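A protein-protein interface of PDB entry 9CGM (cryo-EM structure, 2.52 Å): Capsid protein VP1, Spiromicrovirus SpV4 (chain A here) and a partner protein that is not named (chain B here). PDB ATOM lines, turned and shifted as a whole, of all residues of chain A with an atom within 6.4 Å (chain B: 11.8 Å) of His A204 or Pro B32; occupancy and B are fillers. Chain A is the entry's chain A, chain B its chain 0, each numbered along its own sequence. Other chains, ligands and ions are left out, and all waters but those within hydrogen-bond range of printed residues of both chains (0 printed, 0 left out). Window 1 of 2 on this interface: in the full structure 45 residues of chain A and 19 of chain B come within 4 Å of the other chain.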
ATOM      1  N   ASP A 163     -32.744  11.799  -2.022  1.00  0.00           N
ATOM      2  CA  ASP A 163     -31.455  11.136  -2.150  1.00  0.00           C
ATOM      3  C   ASP A 163     -31.724   9.725  -2.650  1.00  0.00           C
ATOM      4  O   ASP A 163     -32.323   8.913  -1.944  1.00  0.00           O
ATOM      5  CB  ASP A 163     -30.704  11.117  -0.826  1.00  0.00           C
ATOM      6  CG  ASP A 163     -29.343  10.466  -0.942  1.00  0.00           C
ATOM      7  OD1 ASP A 163     -28.458  11.049  -1.598  1.00  0.00           O
ATOM      8  OD2 ASP A 163     -29.150   9.367  -0.386  1.00  0.00           O
ATOM      9  N   LYS A 202     -29.719  16.970   4.761  1.00  0.00           N
ATOM     10  CA  LYS A 202     -28.717  17.926   5.192  1.00  0.00           C
ATOM     11  C   LYS A 202     -27.651  18.097   4.107  1.00  0.00           C
ATOM     12  O   LYS A 202     -27.472  17.247   3.239  1.00  0.00           O
ATOM     13  CB  LYS A 202     -28.134  17.485   6.534  1.00  0.00           C
ATOM     14  CG  LYS A 202     -27.569  16.119   6.489  1.00  0.00           C
ATOM     15  CD  LYS A 202     -27.094  15.620   7.832  1.00  0.00           C
ATOM     16  CE  LYS A 202     -28.227  15.322   8.754  1.00  0.00           C
ATOM     17  NZ  LYS A 202     -27.698  14.681   9.970  1.00  0.00           N
ATOM     18  N   TYR A 203     -26.955  19.231   4.151  1.00  0.00           N
ATOM     19  CA  TYR A 203     -26.060  19.619   3.070  1.00  0.00           C
ATOM     20  C   TYR A 203     -24.934  18.611   2.881  1.00  0.00           C
ATOM     21  O   TYR A 203     -24.537  17.895   3.798  1.00  0.00           O
ATOM     22  CB  TYR A 203     -25.414  20.978   3.321  1.00  0.00           C
ATOM     23  CG  TYR A 203     -26.330  22.162   3.378  1.00  0.00           C
ATOM     24  CD1 TYR A 203     -26.852  22.712   2.224  1.00  0.00           C
ATOM     25  CD2 TYR A 203     -26.593  22.794   4.578  1.00  0.00           C
ATOM     26  CE1 TYR A 203     -27.670  23.810   2.268  1.00  0.00           C
ATOM     27  CE2 TYR A 203     -27.405  23.902   4.634  1.00  0.00           C
ATOM     28  CZ  TYR A 203     -27.938  24.406   3.477  1.00  0.00           C
ATOM     29  OH  TYR A 203     -28.748  25.509   3.524  1.00  0.00           O
ATOM     30  N   HIS A 204     -24.412  18.584   1.660  1.00  0.00           N
ATOM     31  CA  HIS A 204     -23.262  17.753   1.333  1.00  0.00           C
ATOM     32  C   HIS A 204     -22.054  18.139   2.174  1.00  0.00           C
ATOM     33  O   HIS A 204     -21.639  19.298   2.189  1.00  0.00           O
ATOM     34  CB  HIS A 204     -22.928  17.895  -0.149  1.00  0.00           C
ATOM     35  CG  HIS A 204     -23.981  17.365  -1.066  1.00  0.00           C
ATOM     36  ND1 HIS A 204     -24.122  16.024  -1.336  1.00  0.00           N
ATOM     37  CD2 HIS A 204     -24.968  17.992  -1.747  1.00  0.00           C
ATOM     38  CE1 HIS A 204     -25.132  15.849  -2.167  1.00  0.00           C
ATOM     39  NE2 HIS A 204     -25.667  17.026  -2.425  1.00  0.00           N
ATOM     40  N   ASP A 205     -21.483  17.159   2.861  1.00  0.00           N
ATOM     41  CA  ASP A 205     -20.202  17.327   3.528  1.00  0.00           C
ATOM     42  C   ASP A 205     -19.512  15.972   3.500  1.00  0.00           C
ATOM     43  O   ASP A 205     -19.937  15.068   2.777  1.00  0.00           O
ATOM     44  CB  ASP A 205     -20.374  17.924   4.939  1.00  0.00           C
ATOM     45  CG  ASP A 205     -21.038  16.978   5.929  1.00  0.00           C
ATOM     46  OD1 ASP A 205     -21.164  15.773   5.670  1.00  0.00           O
ATOM     47  OD2 ASP A 205     -21.445  17.456   6.999  1.00  0.00           O
ATOM     48  N   TYR A 206     -18.442  15.833   4.279  1.00  0.00           N
ATOM     49  CA  TYR A 206     -17.681  14.590   4.294  1.00  0.00           C
ATOM     50  C   TYR A 206     -18.561  13.387   4.598  1.00  0.00           C
ATOM     51  O   TYR A 206     -18.506  12.379   3.889  1.00  0.00           O
ATOM     52  CB  TYR A 206     -16.548  14.699   5.308  1.00  0.00           C
ATOM     53  CG  TYR A 206     -15.695  13.461   5.449  1.00  0.00           C
ATOM     54  CD1 TYR A 206     -14.777  13.117   4.470  1.00  0.00           C
ATOM     55  CD2 TYR A 206     -15.772  12.667   6.578  1.00  0.00           C
ATOM     56  CE1 TYR A 206     -13.990  12.006   4.601  1.00  0.00           C
ATOM     57  CE2 TYR A 206     -14.986  11.554   6.714  1.00  0.00           C
ATOM     58  CZ  TYR A 206     -14.094  11.229   5.726  1.00  0.00           C
ATOM     59  OH  TYR A 206     -13.301  10.121   5.857  1.00  0.00           O
ATOM     60  N   THR A 208     -22.079  13.246   4.899  1.00  0.00           N
ATOM     61  CA  THR A 208     -23.311  13.177   4.136  1.00  0.00           C
ATOM     62  C   THR A 208     -23.092  12.744   2.699  1.00  0.00           C
ATOM     63  O   THR A 208     -24.065  12.463   1.998  1.00  0.00           O
ATOM     64  CB  THR A 208     -24.012  14.532   4.162  1.00  0.00           C
ATOM     65  OG1 THR A 208     -23.140  15.529   3.629  1.00  0.00           O
ATOM     66  CG2 THR A 208     -24.369  14.898   5.568  1.00  0.00           C
ATOM     67  N   SER A 209     -21.848  12.697   2.242  1.00  0.00           N
ATOM     68  CA  SER A 209     -21.520  12.305   0.885  1.00  0.00           C
ATOM     69  C   SER A 209     -21.081  10.858   0.769  1.00  0.00           C
ATOM     70  O   SER A 209     -20.675  10.436  -0.315  1.00  0.00           O
ATOM     71  CB  SER A 209     -20.447  13.226   0.323  1.00  0.00           C
ATOM     72  OG  SER A 209     -20.975  14.522   0.179  1.00  0.00           O
ATOM     73  N   ARG A 319     -20.829   7.607  -8.528  1.00  0.00           N
ATOM     74  CA  ARG A 319     -20.443   9.007  -8.382  1.00  0.00           C
ATOM     75  C   ARG A 319     -21.550   9.948  -8.831  1.00  0.00           C
ATOM     76  O   ARG A 319     -21.865  10.924  -8.142  1.00  0.00           O
ATOM     77  CB  ARG A 319     -19.179   9.304  -9.183  1.00  0.00           C
ATOM     78  CG  ARG A 319     -17.883   8.837  -8.599  1.00  0.00           C
ATOM     79  CD  ARG A 319     -16.778   9.074  -9.602  1.00  0.00           C
ATOM     80  NE  ARG A 319     -16.917   8.198 -10.756  1.00  0.00           N
ATOM     81  CZ  ARG A 319     -16.157   8.260 -11.838  1.00  0.00           C
ATOM     82  NH1 ARG A 319     -15.222   9.184 -11.933  1.00  0.00           N
ATOM     83  NH2 ARG A 319     -16.348   7.421 -12.834  1.00  0.00           N
ATOM     84  N   GLY A 320     -22.125   9.696  -9.996  1.00  0.00           N
ATOM     85  CA  GLY A 320     -22.915  10.710 -10.652  1.00  0.00           C
ATOM     86  C   GLY A 320     -24.408  10.591 -10.485  1.00  0.00           C
ATOM     87  O   GLY A 320     -25.145  11.528 -10.794  1.00  0.00           O
ATOM     88  N   GLY A 321     -24.868   9.451 -10.015  1.00  0.00           N
ATOM     89  CA  GLY A 321     -26.287   9.212  -9.910  1.00  0.00           C
ATOM     90  C   GLY A 321     -26.834   8.540 -11.155  1.00  0.00           C
ATOM     91  O   GLY A 321     -26.356   8.738 -12.271  1.00  0.00           O
ATOM     92  N   ARG B  20     -17.461  32.414  11.244  1.00  0.00           N
ATOM     93  CA  ARG B  20     -17.767  32.144   9.848  1.00  0.00           C
ATOM     94  C   ARG B  20     -18.883  32.997   9.241  1.00  0.00           C
ATOM     95  O   ARG B  20     -19.913  33.204   9.854  1.00  0.00           O
ATOM     96  CB  ARG B  20     -18.110  30.660   9.682  1.00  0.00           C
ATOM     97  CG  ARG B  20     -18.520  30.278   8.273  1.00  0.00           C
ATOM     98  CD  ARG B  20     -19.018  28.855   8.195  1.00  0.00           C
ATOM     99  NE  ARG B  20     -20.056  28.602   9.178  1.00  0.00           N
ATOM    100  CZ  ARG B  20     -20.452  27.394   9.540  1.00  0.00           C
ATOM    101  NH1 ARG B  20     -19.898  26.328   8.992  1.00  0.00           N
ATOM    102  NH2 ARG B  20     -21.402  27.258  10.452  1.00  0.00           N
ATOM    103  N   ILE B  27     -29.405  29.947  -6.485  1.00  0.00           N
ATOM    104  CA  ILE B  27     -29.373  28.497  -6.552  1.00  0.00           C
ATOM    105  C   ILE B  27     -29.426  28.081  -8.011  1.00  0.00           C
ATOM    106  O   ILE B  27     -30.204  28.632  -8.796  1.00  0.00           O
ATOM    107  CB  ILE B  27     -30.533  27.886  -5.753  1.00  0.00           C
ATOM    108  CG1 ILE B  27     -30.383  28.234  -4.275  1.00  0.00           C
ATOM    109  CG2 ILE B  27     -30.577  26.385  -5.949  1.00  0.00           C
ATOM    110  CD1 ILE B  27     -31.567  27.878  -3.443  1.00  0.00           C
ATOM    111  N   MET B  28     -28.581  27.133  -8.381  1.00  0.00           N
ATOM    112  CA  MET B  28     -28.568  26.549  -9.707  1.00  0.00           C
ATOM    113  C   MET B  28     -28.656  25.040  -9.588  1.00  0.00           C
ATOM    114  O   MET B  28     -28.200  24.464  -8.597  1.00  0.00           O
ATOM    115  CB  MET B  28     -27.295  26.925 -10.476  1.00  0.00           C
ATOM    116  CG  MET B  28     -27.152  28.404 -10.748  1.00  0.00           C
ATOM    117  SD  MET B  28     -28.460  29.017 -11.821  1.00  0.00           S
ATOM    118  CE  MET B  28     -28.051  30.755 -11.884  1.00  0.00           C
ATOM    119  N   PRO B  29     -29.253  24.373 -10.573  1.00  0.00           N
ATOM    120  CA  PRO B  29     -29.200  22.907 -10.600  1.00  0.00           C
ATOM    121  C   PRO B  29     -27.767  22.438 -10.798  1.00  0.00           C
ATOM    122  O   PRO B  29     -27.053  22.931 -11.670  1.00  0.00           O
ATOM    123  CB  PRO B  29     -30.097  22.544 -11.786  1.00  0.00           C
ATOM    124  CG  PRO B  29     -30.100  23.758 -12.635  1.00  0.00           C
ATOM    125  CD  PRO B  29     -30.019  24.915 -11.705  1.00  0.00           C
ATOM    126  N   SER B  30     -27.346  21.490  -9.974  1.00  0.00           N
ATOM    127  CA  SER B  30     -25.987  20.981  -9.990  1.00  0.00           C
ATOM    128  C   SER B  30     -26.021  19.471  -9.852  1.00  0.00           C
ATOM    129  O   SER B  30     -27.053  18.880  -9.544  1.00  0.00           O
ATOM    130  CB  SER B  30     -25.144  21.598  -8.872  1.00  0.00           C
ATOM    131  OG  SER B  30     -25.649  21.243  -7.599  1.00  0.00           O
ATOM    132  N   ASN B  31     -24.872  18.846 -10.089  1.00  0.00           N
ATOM    133  CA  ASN B  31     -24.718  17.397  -9.980  1.00  0.00           C
ATOM    134  C   ASN B  31     -23.590  17.089  -9.012  1.00  0.00           C
ATOM    135  O   ASN B  31     -22.459  16.814  -9.427  1.00  0.00           O
ATOM    136  CB  ASN B  31     -24.447  16.766 -11.342  1.00  0.00           C
ATOM    137  CG  ASN B  31     -25.658  16.772 -12.225  1.00  0.00           C
ATOM    138  OD1 ASN B  31     -26.560  15.961 -12.051  1.00  0.00           O
ATOM    139  ND2 ASN B  31     -25.696  17.693 -13.175  1.00  0.00           N
ATOM    140  N   PRO B  32     -23.859  17.127  -7.722  1.00  0.00           N
ATOM    141  CA  PRO B  32     -22.820  16.774  -6.750  1.00  0.00           C
ATOM    142  C   PRO B  32     -22.612  15.275  -6.669  1.00  0.00           C
ATOM    143  O   PRO B  32     -23.196  14.518  -7.446  1.00  0.00           O
ATOM    144  CB  PRO B  32     -23.367  17.344  -5.441  1.00  0.00           C
ATOM    145  CG  PRO B  32     -24.829  17.321  -5.623  1.00  0.00           C
ATOM    146  CD  PRO B  32     -25.098  17.573  -7.065  1.00  0.00           C
ATOM    147  N   ARG B  33     -21.779  14.839  -5.736  1.00  0.00           N
ATOM    148  CA  ARG B  33     -21.501  13.422  -5.566  1.00  0.00           C
ATOM    149  C   ARG B  33     -22.774  12.657  -5.229  1.00  0.00           C
ATOM    150  O   ARG B  33     -23.478  12.988  -4.272  1.00  0.00           O
ATOM    151  CB  ARG B  33     -20.453  13.234  -4.471  1.00  0.00           C
ATOM    152  CG  ARG B  33     -20.097  11.801  -4.155  1.00  0.00           C
ATOM    153  CD  ARG B  33     -19.036  11.741  -3.080  1.00  0.00           C
ATOM    154  NE  ARG B  33     -18.808  10.384  -2.595  1.00  0.00           N
ATOM    155  CZ  ARG B  33     -18.021   9.490  -3.180  1.00  0.00           C
ATOM    156  NH1 ARG B  33     -17.377   9.791  -4.294  1.00  0.00           N
ATOM    157  NH2 ARG B  33     -17.891   8.286  -2.652  1.00  0.00           N
ATOM    158  N   GLY B  34     -23.065  11.629  -6.021  1.00  0.00           N
ATOM    159  CA  GLY B  34     -24.173  10.741  -5.764  1.00  0.00           C
ATOM    160  C   GLY B  34     -25.505  11.155  -6.340  1.00  0.00           C
ATOM    161  O   GLY B  34     -26.531  10.620  -5.917  1.00  0.00           O
ATOM    162  N   GLY B  35     -25.531  12.086  -7.275  1.00  0.00           N
ATOM    163  CA  GLY B  35     -26.766  12.503  -7.906  1.00  0.00           C
ATOM    164  C   GLY B  35     -27.230  13.853  -7.395  1.00  0.00           C
ATOM    165  O   GLY B  35     -26.634  14.459  -6.506  1.00  0.00           O
ATOM    166  N   ARG B  36     -28.327  14.312  -7.982  1.00  0.00           N
ATOM    167  CA  ARG B  36     -28.908  15.598  -7.622  1.00  0.00           C
ATOM    168  C   ARG B  36     -29.711  15.494  -6.336  1.00  0.00           C
ATOM    169  O   ARG B  36     -30.630  14.680  -6.233  1.00  0.00           O
ATOM    170  CB  ARG B  36     -29.821  16.109  -8.733  1.00  0.00           C
ATOM    171  CG  ARG B  36     -29.128  16.521  -9.994  1.00  0.00           C
ATOM    172  CD  ARG B  36     -30.145  17.052 -10.974  1.00  0.00           C
ATOM    173  NE  ARG B  36     -29.531  17.505 -12.212  1.00  0.00           N
ATOM    174  CZ  ARG B  36     -30.209  17.918 -13.274  1.00  0.00           C
ATOM    175  NH1 ARG B  36     -31.526  17.930 -13.260  1.00  0.00           N
ATOM    176  NH2 ARG B  36     -29.567  18.317 -14.356  1.00  0.00           N
ATOM    177  N   ARG B  37     -29.378  16.330  -5.360  1.00  0.00           N
ATOM    178  CA  ARG B  37     -30.323  16.597  -4.290  1.00  0.00           C
ATOM    179  C   ARG B  37     -30.079  18.016  -3.808  1.00  0.00           C
ATOM    180  O   ARG B  37     -28.938  18.471  -3.744  1.00  0.00           O
ATOM    181  CB  ARG B  37     -30.199  15.586  -3.143  1.00  0.00           C
ATOM    182  CG  ARG B  37     -28.982  15.774  -2.325  1.00  0.00           C
ATOM    183  CD  ARG B  37     -28.786  14.731  -1.284  1.00  0.00           C
ATOM    184  NE  ARG B  37     -27.708  15.166  -0.411  1.00  0.00           N
ATOM    185  CZ  ARG B  37     -27.013  14.375   0.386  1.00  0.00           C
ATOM    186  NH1 ARG B  37     -27.225  13.073   0.367  1.00  0.00           N
ATOM    187  NH2 ARG B  37     -26.065  14.886   1.148  1.00  0.00           N
ATOM    188  N   PHE B  38     -31.154  18.712  -3.488  1.00  0.00           N
ATOM    189  CA  PHE B  38     -31.073  20.093  -3.044  1.00  0.00           C
ATOM    190  C   PHE B  38     -30.921  20.252  -1.541  1.00  0.00           C
ATOM    191  O   PHE B  38     -30.082  21.020  -1.079  1.00  0.00           O
ATOM    192  CB  PHE B  38     -32.305  20.847  -3.506  1.00  0.00           C
ATOM    193  CG  PHE B  38     -32.198  21.414  -4.872  1.00  0.00           C
ATOM    194  CD1 PHE B  38     -30.973  21.748  -5.416  1.00  0.00           C
ATOM    195  CD2 PHE B  38     -33.335  21.646  -5.618  1.00  0.00           C
ATOM    196  CE1 PHE B  38     -30.898  22.295  -6.678  1.00  0.00           C
ATOM    197  CE2 PHE B  38     -33.263  22.185  -6.868  1.00  0.00           C
ATOM    198  CZ  PHE B  38     -32.049  22.515  -7.409  1.00  0.00           C
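Among the printed residues, merely in contact across the chains: His A204 with Pro B32, Gly A320 with Gly B35, Arg A319 with Arg B33, Gly A321 with Gly B35, Arg A319 with Pro B32, His A204 with Arg B33 and Arg A319 with Gly B35.
The guanidinium group (NH1) of Arg B37 lies within salt-bridge range of the side-chain carboxylate (OD1) of Asp A163.
The guanidinium group (NH2) of Arg B37 sits at hydrogen-bond distance from the backbone carbonyl oxygen (O) of Lys A202, at 3.5 Å.
ND1 of His A204 lies within hydrogen-bond range of NH2 of Arg B37 (3.4 Å).
The guanidinium group of Arg B37 sits at hydrogen-bond distance from the backbone carbonyl oxygen of Thr A208, 3.3 Å away.
The guanidinium group (NE) of Arg B33 sits at hydrogen-bond distance from the backbone carbonyl oxygen (O) of Ser A209 (2.9 Å).
The backbone NH (N) of Gly B34 is in hydrogen-bond range of the backbone carbonyl oxygen (O) of Arg A319, at 2.5 Å.
Of the 11 printed residues of chain A, 8 touch a printed residue of chain B.
Hydrophobic or aromatic side chains of chain A within 4 Å of the printed part of chain B: His A204.
Of the 13 printed residues of chain B, 5 touch a printed residue of chain A.
Hydrophobic or aromatic side chains of chain B that line the printed part of chain A: Pro B32.
Among the printed residues, 13 pairs touch across the chains.
Among the printed residues, Asp or Glu carboxylates within 4 Å of a Lys or Arg side-chain nitrogen of the other chain: Asp A163 with Arg B37.
Of the printed residues of chain B, Asp A163 touches Arg B37.
His A204 touches just these residues of chain B: Pro B32 (3.3 Å), Arg B33 (3.9 Å) and Arg B37 (3.2 Å).
No residue of chain B comes within 4 Å of Asp A205.
Ser A209 touches just one residue of chain B: Arg B33 (2.9 Å).
Gly A320 touches just one residue of chain B: Gly B35.
Pro B32 touches just these residues of chain A: His A204 and Arg A319.
Printed residues of chain A within 4 Å of Gly B34: Arg A319.
Of the printed residues of chain A, Arg B37 touches Asp A163 (3.1 Å), Lys A202 (3.5 Å), His A204 (3.2 Å) and Thr A208 (3.3 Å).
The nearest residue of chain A that does not touch Pro B32 is Gly A320 (4.9 Å).
The backbone carbonyl oxygen (O) of Tyr A203 sits at hydrogen-bond distance from the side-chain hydroxyl (OG1) of Thr A208 (2.8 Å).
The backbone NH (N) of Asp A205 sits at hydrogen-bond distance from the side-chain hydroxyl (OG1) of Thr A208 (2.4 Å).
The backbone carbonyl oxygen (O) of Asp A205 is in hydrogen-bond range of the side-chain hydroxyl (OG) of Ser A209 (2.9 Å).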
